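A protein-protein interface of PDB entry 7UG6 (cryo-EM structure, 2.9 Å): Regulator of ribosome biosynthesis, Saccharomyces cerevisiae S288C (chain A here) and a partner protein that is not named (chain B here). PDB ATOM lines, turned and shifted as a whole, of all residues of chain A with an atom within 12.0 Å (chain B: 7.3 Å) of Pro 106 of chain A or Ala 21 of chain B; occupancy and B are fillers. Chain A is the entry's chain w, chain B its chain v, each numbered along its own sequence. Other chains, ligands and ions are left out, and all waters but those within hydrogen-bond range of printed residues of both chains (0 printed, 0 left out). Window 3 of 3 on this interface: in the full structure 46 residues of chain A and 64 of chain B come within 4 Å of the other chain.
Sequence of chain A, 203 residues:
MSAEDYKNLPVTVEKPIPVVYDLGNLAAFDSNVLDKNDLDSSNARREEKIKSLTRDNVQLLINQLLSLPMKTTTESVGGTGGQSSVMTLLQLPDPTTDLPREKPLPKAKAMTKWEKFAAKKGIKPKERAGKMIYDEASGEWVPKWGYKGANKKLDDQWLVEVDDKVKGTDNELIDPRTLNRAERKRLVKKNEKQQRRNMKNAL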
ATOM      1  N   ARG A 101       6.511  22.807 -14.158  1.00  0.00           N
ATOM      2  CA  ARG A 101       6.507  21.368 -14.254  1.00  0.00           C
ATOM      3  C   ARG A 101       7.877  20.886 -14.684  1.00  0.00           C
ATOM      4  O   ARG A 101       8.747  21.665 -15.073  1.00  0.00           O
ATOM      5  CB  ARG A 101       5.459  20.896 -15.248  1.00  0.00           C
ATOM      6  CG  ARG A 101       4.098  20.728 -14.664  1.00  0.00           C
ATOM      7  CD  ARG A 101       3.163  20.250 -15.720  1.00  0.00           C
ATOM      8  NE  ARG A 101       3.603  18.985 -16.291  1.00  0.00           N
ATOM      9  CZ  ARG A 101       3.140  17.800 -15.911  1.00  0.00           C
ATOM     10  NH1 ARG A 101       2.213  17.724 -14.972  1.00  0.00           N
ATOM     11  NH2 ARG A 101       3.595  16.693 -16.474  1.00  0.00           N
ATOM     12  N   GLU A 102       8.068  19.576 -14.606  1.00  0.00           N
ATOM     13  CA  GLU A 102       9.336  19.014 -15.038  1.00  0.00           C
ATOM     14  C   GLU A 102       9.325  18.735 -16.526  1.00  0.00           C
ATOM     15  O   GLU A 102      10.241  19.144 -17.244  1.00  0.00           O
ATOM     16  CB  GLU A 102       9.634  17.749 -14.252  1.00  0.00           C
ATOM     17  CG  GLU A 102      10.961  17.140 -14.583  1.00  0.00           C
ATOM     18  CD  GLU A 102      11.249  15.918 -13.744  1.00  0.00           C
ATOM     19  OE1 GLU A 102      10.389  15.551 -12.916  1.00  0.00           O
ATOM     20  OE2 GLU A 102      12.331  15.315 -13.916  1.00  0.00           O
ATOM     21  N   LYS A 103       8.300  18.052 -17.010  1.00  0.00           N
ATOM     22  CA  LYS A 103       8.190  17.673 -18.407  1.00  0.00           C
ATOM     23  C   LYS A 103       6.826  18.096 -18.923  1.00  0.00           C
ATOM     24  O   LYS A 103       5.884  18.257 -18.142  1.00  0.00           O
ATOM     25  CB  LYS A 103       8.382  16.164 -18.593  1.00  0.00           C
ATOM     26  CG  LYS A 103       9.478  15.593 -17.736  1.00  0.00           C
ATOM     27  CD  LYS A 103       9.863  14.207 -18.168  1.00  0.00           C
ATOM     28  CE  LYS A 103      11.084  13.751 -17.404  1.00  0.00           C
ATOM     29  NZ  LYS A 103      10.709  13.096 -16.124  1.00  0.00           N
ATOM     30  N   PRO A 104       6.695  18.307 -20.231  1.00  0.00           N
ATOM     31  CA  PRO A 104       5.385  18.634 -20.797  1.00  0.00           C
ATOM     32  C   PRO A 104       4.400  17.502 -20.616  1.00  0.00           C
ATOM     33  O   PRO A 104       4.807  16.351 -20.467  1.00  0.00           O
ATOM     34  CB  PRO A 104       5.692  18.874 -22.278  1.00  0.00           C
ATOM     35  CG  PRO A 104       7.017  18.279 -22.498  1.00  0.00           C
ATOM     36  CD  PRO A 104       7.754  18.452 -21.234  1.00  0.00           C
ATOM     37  N   LEU A 105       3.110  17.823 -20.620  1.00  0.00           N
ATOM     38  CA  LEU A 105       2.086  16.832 -20.348  1.00  0.00           C
ATOM     39  C   LEU A 105       2.129  15.723 -21.396  1.00  0.00           C
ATOM     40  O   LEU A 105       2.446  15.973 -22.561  1.00  0.00           O
ATOM     41  CB  LEU A 105       0.710  17.480 -20.332  1.00  0.00           C
ATOM     42  CG  LEU A 105       0.241  18.092 -19.016  1.00  0.00           C
ATOM     43  CD1 LEU A 105       0.160  17.023 -17.955  1.00  0.00           C
ATOM     44  CD2 LEU A 105       1.134  19.208 -18.561  1.00  0.00           C
ATOM     45  N   PRO A 106       1.796  14.491 -21.014  1.00  0.00           N
ATOM     46  CA  PRO A 106       2.074  13.346 -21.890  1.00  0.00           C
ATOM     47  C   PRO A 106       1.113  13.221 -23.058  1.00  0.00           C
ATOM     48  O   PRO A 106       1.026  12.156 -23.678  1.00  0.00           O
ATOM     49  CB  PRO A 106       1.943  12.153 -20.941  1.00  0.00           C
ATOM     50  CG  PRO A 106       0.906  12.588 -19.986  1.00  0.00           C
ATOM     51  CD  PRO A 106       1.145  14.062 -19.765  1.00  0.00           C
ATOM     52  N   LYS A 107       0.380  14.294 -23.362  1.00  0.00           N
ATOM     53  CA  LYS A 107      -0.630  14.284 -24.414  1.00  0.00           C
ATOM     54  C   LYS A 107      -0.078  13.946 -25.796  1.00  0.00           C
ATOM     55  O   LYS A 107      -0.872  13.720 -26.715  1.00  0.00           O
ATOM     56  CB  LYS A 107      -1.316  15.646 -24.478  1.00  0.00           C
ATOM     57  CG  LYS A 107      -0.371  16.758 -24.889  1.00  0.00           C
ATOM     58  CD  LYS A 107      -1.075  18.092 -25.026  1.00  0.00           C
ATOM     59  CE  LYS A 107      -1.427  18.683 -23.679  1.00  0.00           C
ATOM     60  NZ  LYS A 107      -1.960  20.067 -23.820  1.00  0.00           N
ATOM     61  N   ALA A 108       1.246  13.883 -25.962  1.00  0.00           N
ATOM     62  CA  ALA A 108       1.860  13.782 -27.282  1.00  0.00           C
ATOM     63  C   ALA A 108       1.528  12.487 -28.014  1.00  0.00           C
ATOM     64  O   ALA A 108       1.774  12.404 -29.221  1.00  0.00           O
ATOM     65  CB  ALA A 108       3.377  13.931 -27.162  1.00  0.00           C
ATOM     66  N   LYS A 109       0.981  11.486 -27.325  1.00  0.00           N
ATOM     67  CA  LYS A 109       0.567  10.248 -27.976  1.00  0.00           C
ATOM     68  C   LYS A 109      -0.616  10.508 -28.903  1.00  0.00           C
ATOM     69  O   LYS A 109      -1.633  11.073 -28.486  1.00  0.00           O
ATOM     70  CB  LYS A 109       0.209   9.211 -26.914  1.00  0.00           C
ATOM     71  CG  LYS A 109       0.184   7.772 -27.384  1.00  0.00           C
ATOM     72  CD  LYS A 109      -0.142   6.865 -26.205  1.00  0.00           C
ATOM     73  CE  LYS A 109      -0.135   5.399 -26.589  1.00  0.00           C
ATOM     74  NZ  LYS A 109      -0.415   4.549 -25.402  1.00  0.00           N
ATOM     75  N   ALA A 110      -0.489  10.071 -30.154  1.00  0.00           N
ATOM     76  CA  ALA A 110      -1.405  10.458 -31.216  1.00  0.00           C
ATOM     77  C   ALA A 110      -2.558   9.460 -31.339  1.00  0.00           C
ATOM     78  O   ALA A 110      -2.830   8.663 -30.437  1.00  0.00           O
ATOM     79  CB  ALA A 110      -0.650  10.590 -32.537  1.00  0.00           C
ATOM     80  N   MET A 111      -3.253   9.520 -32.477  1.00  0.00           N
ATOM     81  CA  MET A 111      -4.437   8.712 -32.742  1.00  0.00           C
ATOM     82  C   MET A 111      -4.263   7.986 -34.070  1.00  0.00           C
ATOM     83  O   MET A 111      -3.878   8.599 -35.069  1.00  0.00           O
ATOM     84  CB  MET A 111      -5.687   9.603 -32.724  1.00  0.00           C
ATOM     85  CG  MET A 111      -7.026   8.918 -32.920  1.00  0.00           C
ATOM     86  SD  MET A 111      -7.455   8.598 -34.630  1.00  0.00           S
ATOM     87  CE  MET A 111      -7.821  10.264 -35.179  1.00  0.00           C
ATOM     88  N   LEU B  16      12.228   3.480 -18.610  1.00  0.00           N
ATOM     89  CA  LEU B  16      11.741   4.445 -19.587  1.00  0.00           C
ATOM     90  C   LEU B  16      10.401   5.021 -19.162  1.00  0.00           C
ATOM     91  O   LEU B  16      10.143   6.214 -19.351  1.00  0.00           O
ATOM     92  CB  LEU B  16      11.628   3.791 -20.962  1.00  0.00           C
ATOM     93  CG  LEU B  16      12.847   3.667 -21.884  1.00  0.00           C
ATOM     94  CD1 LEU B  16      13.335   5.041 -22.281  1.00  0.00           C
ATOM     95  CD2 LEU B  16      13.979   2.872 -21.265  1.00  0.00           C
ATOM     96  N   VAL B  17       9.535   4.188 -18.587  1.00  0.00           N
ATOM     97  CA  VAL B  17       8.240   4.659 -18.111  1.00  0.00           C
ATOM     98  C   VAL B  17       8.406   5.610 -16.937  1.00  0.00           C
ATOM     99  O   VAL B  17       7.745   6.650 -16.868  1.00  0.00           O
ATOM    100  CB  VAL B  17       7.340   3.466 -17.754  1.00  0.00           C
ATOM    101  CG1 VAL B  17       6.115   3.936 -17.015  1.00  0.00           C
ATOM    102  CG2 VAL B  17       6.928   2.744 -19.019  1.00  0.00           C
ATOM    103  N   LYS B  18       9.287   5.276 -15.998  1.00  0.00           N
ATOM    104  CA  LYS B  18       9.503   6.154 -14.857  1.00  0.00           C
ATOM    105  C   LYS B  18      10.076   7.488 -15.301  1.00  0.00           C
ATOM    106  O   LYS B  18       9.817   8.523 -14.680  1.00  0.00           O
ATOM    107  CB  LYS B  18      10.431   5.488 -13.850  1.00  0.00           C
ATOM    108  CG  LYS B  18      10.274   5.999 -12.430  1.00  0.00           C
ATOM    109  CD  LYS B  18       8.881   5.722 -11.884  1.00  0.00           C
ATOM    110  CE  LYS B  18       8.899   5.629 -10.366  1.00  0.00           C
ATOM    111  NZ  LYS B  18       7.752   4.849  -9.831  1.00  0.00           N
ATOM    112  N   ARG B  19      10.867   7.485 -16.372  1.00  0.00           N
ATOM    113  CA  ARG B  19      11.413   8.741 -16.865  1.00  0.00           C
ATOM    114  C   ARG B  19      10.371   9.561 -17.613  1.00  0.00           C
ATOM    115  O   ARG B  19      10.285  10.775 -17.419  1.00  0.00           O
ATOM    116  CB  ARG B  19      12.630   8.481 -17.743  1.00  0.00           C
ATOM    117  CG  ARG B  19      13.861   8.112 -16.941  1.00  0.00           C
ATOM    118  CD  ARG B  19      15.141   8.490 -17.665  1.00  0.00           C
ATOM    119  NE  ARG B  19      15.440   7.596 -18.775  1.00  0.00           N
ATOM    120  CZ  ARG B  19      15.390   7.949 -20.053  1.00  0.00           C
ATOM    121  NH1 ARG B  19      15.041   9.181 -20.388  1.00  0.00           N
ATOM    122  NH2 ARG B  19      15.687   7.068 -20.998  1.00  0.00           N
ATOM    123  N   GLU B  20       9.560   8.923 -18.452  1.00  0.00           N
ATOM    124  CA  GLU B  20       8.714   9.670 -19.377  1.00  0.00           C
ATOM    125  C   GLU B  20       7.585  10.383 -18.645  1.00  0.00           C
ATOM    126  O   GLU B  20       7.278  10.076 -17.493  1.00  0.00           O
ATOM    127  CB  GLU B  20       8.159   8.742 -20.461  1.00  0.00           C
ATOM    128  CG  GLU B  20       7.282   7.603 -19.984  1.00  0.00           C
ATOM    129  CD  GLU B  20       5.836   7.988 -19.824  1.00  0.00           C
ATOM    130  OE1 GLU B  20       5.420   9.004 -20.418  1.00  0.00           O
ATOM    131  OE2 GLU B  20       5.109   7.273 -19.110  1.00  0.00           O
ATOM    132  N   ALA B  21       6.960  11.330 -19.342  1.00  0.00           N
ATOM    133  CA  ALA B  21       6.110  12.332 -18.713  1.00  0.00           C
ATOM    134  C   ALA B  21       4.895  11.711 -18.043  1.00  0.00           C
ATOM    135  O   ALA B  21       4.361  10.695 -18.486  1.00  0.00           O
ATOM    136  CB  ALA B  21       5.653  13.351 -19.749  1.00  0.00           C
ATOM    137  N   LYS B  22       4.452  12.341 -16.962  1.00  0.00           N
ATOM    138  CA  LYS B  22       3.336  11.839 -16.183  1.00  0.00           C
ATOM    139  C   LYS B  22       2.405  12.983 -15.830  1.00  0.00           C
ATOM    140  O   LYS B  22       2.792  14.154 -15.825  1.00  0.00           O
ATOM    141  CB  LYS B  22       3.817  11.117 -14.923  1.00  0.00           C
ATOM    142  CG  LYS B  22       4.514   9.814 -15.234  1.00  0.00           C
ATOM    143  CD  LYS B  22       4.991   9.105 -13.998  1.00  0.00           C
ATOM    144  CE  LYS B  22       5.539   7.753 -14.378  1.00  0.00           C
ATOM    145  NZ  LYS B  22       6.736   7.908 -15.237  1.00  0.00           N
ATOM    146  N   LEU B  23       1.150  12.626 -15.558  1.00  0.00           N
ATOM    147  CA  LEU B  23       0.158  13.622 -15.182  1.00  0.00           C
ATOM    148  C   LEU B  23       0.523  14.282 -13.864  1.00  0.00           C
ATOM    149  O   LEU B  23       0.567  15.511 -13.763  1.00  0.00           O
ATOM    150  CB  LEU B  23      -1.214  12.970 -15.095  1.00  0.00           C
ATOM    151  CG  LEU B  23      -1.718  12.477 -16.439  1.00  0.00           C
ATOM    152  CD1 LEU B  23      -3.018  11.711 -16.293  1.00  0.00           C
ATOM    153  CD2 LEU B  23      -1.897  13.668 -17.342  1.00  0.00           C
ATOM    154  N   VAL B  24       0.781  13.480 -12.841  1.00  0.00           N
ATOM    155  CA  VAL B  24       1.299  13.962 -11.571  1.00  0.00           C
ATOM    156  C   VAL B  24       2.767  13.583 -11.523  1.00  0.00           C
ATOM    157  O   VAL B  24       3.111  12.422 -11.272  1.00  0.00           O
ATOM    158  CB  VAL B  24       0.533  13.383 -10.378  1.00  0.00           C
ATOM    159  CG1 VAL B  24       0.958  14.082  -9.114  1.00  0.00           C
ATOM    160  CG2 VAL B  24      -0.956  13.535 -10.593  1.00  0.00           C
ATOM    161  N   GLU B  25       3.626  14.558 -11.775  1.00  0.00           N
ATOM    162  CA  GLU B  25       5.031  14.292 -11.997  1.00  0.00           C
ATOM    163  C   GLU B  25       5.710  13.883 -10.700  1.00  0.00           C
ATOM    164  O   GLU B  25       5.267  14.233  -9.604  1.00  0.00           O
ATOM    165  CB  GLU B  25       5.691  15.528 -12.613  1.00  0.00           C
ATOM    166  CG  GLU B  25       7.153  15.378 -12.939  1.00  0.00           C
ATOM    167  CD  GLU B  25       7.413  14.346 -14.015  1.00  0.00           C
ATOM    168  OE1 GLU B  25       6.515  14.094 -14.845  1.00  0.00           O
ATOM    169  OE2 GLU B  25       8.521  13.772 -14.020  1.00  0.00           O
ATOM    170  N   TYR B 108      13.579  18.654 -21.331  1.00  0.00           N
ATOM    171  CA  TYR B 108      14.986  18.517 -21.019  1.00  0.00           C
ATOM    172  C   TYR B 108      15.788  19.736 -21.438  1.00  0.00           C
ATOM    173  O   TYR B 108      16.979  19.810 -21.129  1.00  0.00           O
ATOM    174  CB  TYR B 108      15.556  17.257 -21.667  1.00  0.00           C
ATOM    175  CG  TYR B 108      15.084  16.004 -20.982  1.00  0.00           C
ATOM    176  CD1 TYR B 108      15.351  15.784 -19.647  1.00  0.00           C
ATOM    177  CD2 TYR B 108      14.369  15.041 -21.668  1.00  0.00           C
ATOM    178  CE1 TYR B 108      14.915  14.646 -19.012  1.00  0.00           C
ATOM    179  CE2 TYR B 108      13.936  13.896 -21.038  1.00  0.00           C
ATOM    180  CZ  TYR B 108      14.214  13.707 -19.711  1.00  0.00           C
ATOM    181  OH  TYR B 108      13.790  12.571 -19.075  1.00  0.00           O
ATOM    182  N   PRO B 252      -2.792  19.288 -15.723  1.00  0.00           N
ATOM    183  CA  PRO B 252      -3.027  18.011 -16.413  1.00  0.00           C
ATOM    184  C   PRO B 252      -4.422  17.880 -16.994  1.00  0.00           C
ATOM    185  O   PRO B 252      -4.627  17.044 -17.883  1.00  0.00           O
ATOM    186  CB  PRO B 252      -2.786  16.960 -15.324  1.00  0.00           C
ATOM    187  CG  PRO B 252      -2.292  17.693 -14.122  1.00  0.00           C
ATOM    188  CD  PRO B 252      -2.088  19.122 -14.446  1.00  0.00           C
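O of Arg 19 of chain B lies within hydrogen-bond range of NZ of Lys 103 of chain A, 2.7 Å away. O of Lys 22 of chain B lies within hydrogen-bond range of NH2 of Arg 101 of chain A (2.7 Å). NH1 of Arg 101 of chain A lies within hydrogen-bond range of O of Leu 23 of chain B (3.0 Å). The side-chain amino group (NZ) of Lys 103 of chain A is in salt-bridge range of the side-chain carboxylate (OE2) of Glu 25 of chain B, 3.1 Å away. OE1 of Glu 102 of chain A lies close to OE2 of Glu 25 of chain B, 2.8 Å away.
Of the 12 printed residues of chain B, 7 touch a printed residue of chain A. Of the 11 printed residues of chain A, 6 touch a printed residue of chain B. Hydrophobic or aromatic side chains of chain A within 4 Å of the printed part of chain B: Leu 105 and Pro 106. Along chain A the printed residues that touch a printed residue of chain B span positions 101 to 106. Among the printed residues, 11 pairs touch across the chains. Among the printed residues, Asp or Glu carboxylates within 4 Å of a Lys or Arg side-chain nitrogen of the other chain: Lys 103 of chain A with Glu 25 of chain B (3.1 Å).
O of Lys 18 of chain B lies within hydrogen-bond range of NZ of Lys 22 of chain B. O of Glu 20 of chain B lies within hydrogen-bond range of NZ of Lys 22 of chain B, 3.2 Å away. The side-chain carboxylate (OE1) of Glu 25 of chain B lies within hydrogen-bond range of the backbone NH (N) of Lys 22 of chain B, at 3.4 Å. O of Lys 103 of chain A sits at hydrogen-bond distance from NE of Arg 101 of chain A (3.0 Å). NZ of Lys 103 of chain A is in salt-bridge range of OE2 of Glu 102 of chain A, 3.5 Å away.
Printed residues of chain B within 4 Å of Pro 106 of chain A: Ala 21 (3.7 Å) and Leu 23 (3.9 Å). Of chain A, only Pro 104 and Pro 106 come within 4 Å of Ala 21 of chain B. Lys 22 of chain B touches just one residue of chain A: Arg 101 (2.7 Å). Printed residues of chain B within 4 Å of Pro 104 of chain A: Ala 21 (3.2 Å). Of the printed residues of chain B, Arg 101 of chain A touches Lys 22 and Leu 23. Val 17 of chain B touches none of the printed residues of chain A. The nearest residue of chain B that does not touch Pro 106 of chain A is Lys 22 of chain B (4.3 Å). The nearest printed residue of chain A that does not touch Arg 19 of chain B is Glu 102 of chain A (6.1 Å).
Tyr 108 of chain B touches Lys 103 of chain A. Ala 21 of chain B touches Pro 104 of chain A (CB to O, 3.2 Å). CD1 of Leu 105 of chain A touches CD2 of Leu 23 of chain B, at 3.98 Å. Pro 252 of chain B touches Leu 105 of chain A (CA to CD1, 3.7 Å). CB of Pro 106 of chain A touches O of Ala 21 of chain B, 3.7 Å away. CD of Pro 106 of chain A touches CD2 of Leu 23 of chain B, at 3.9 Å.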
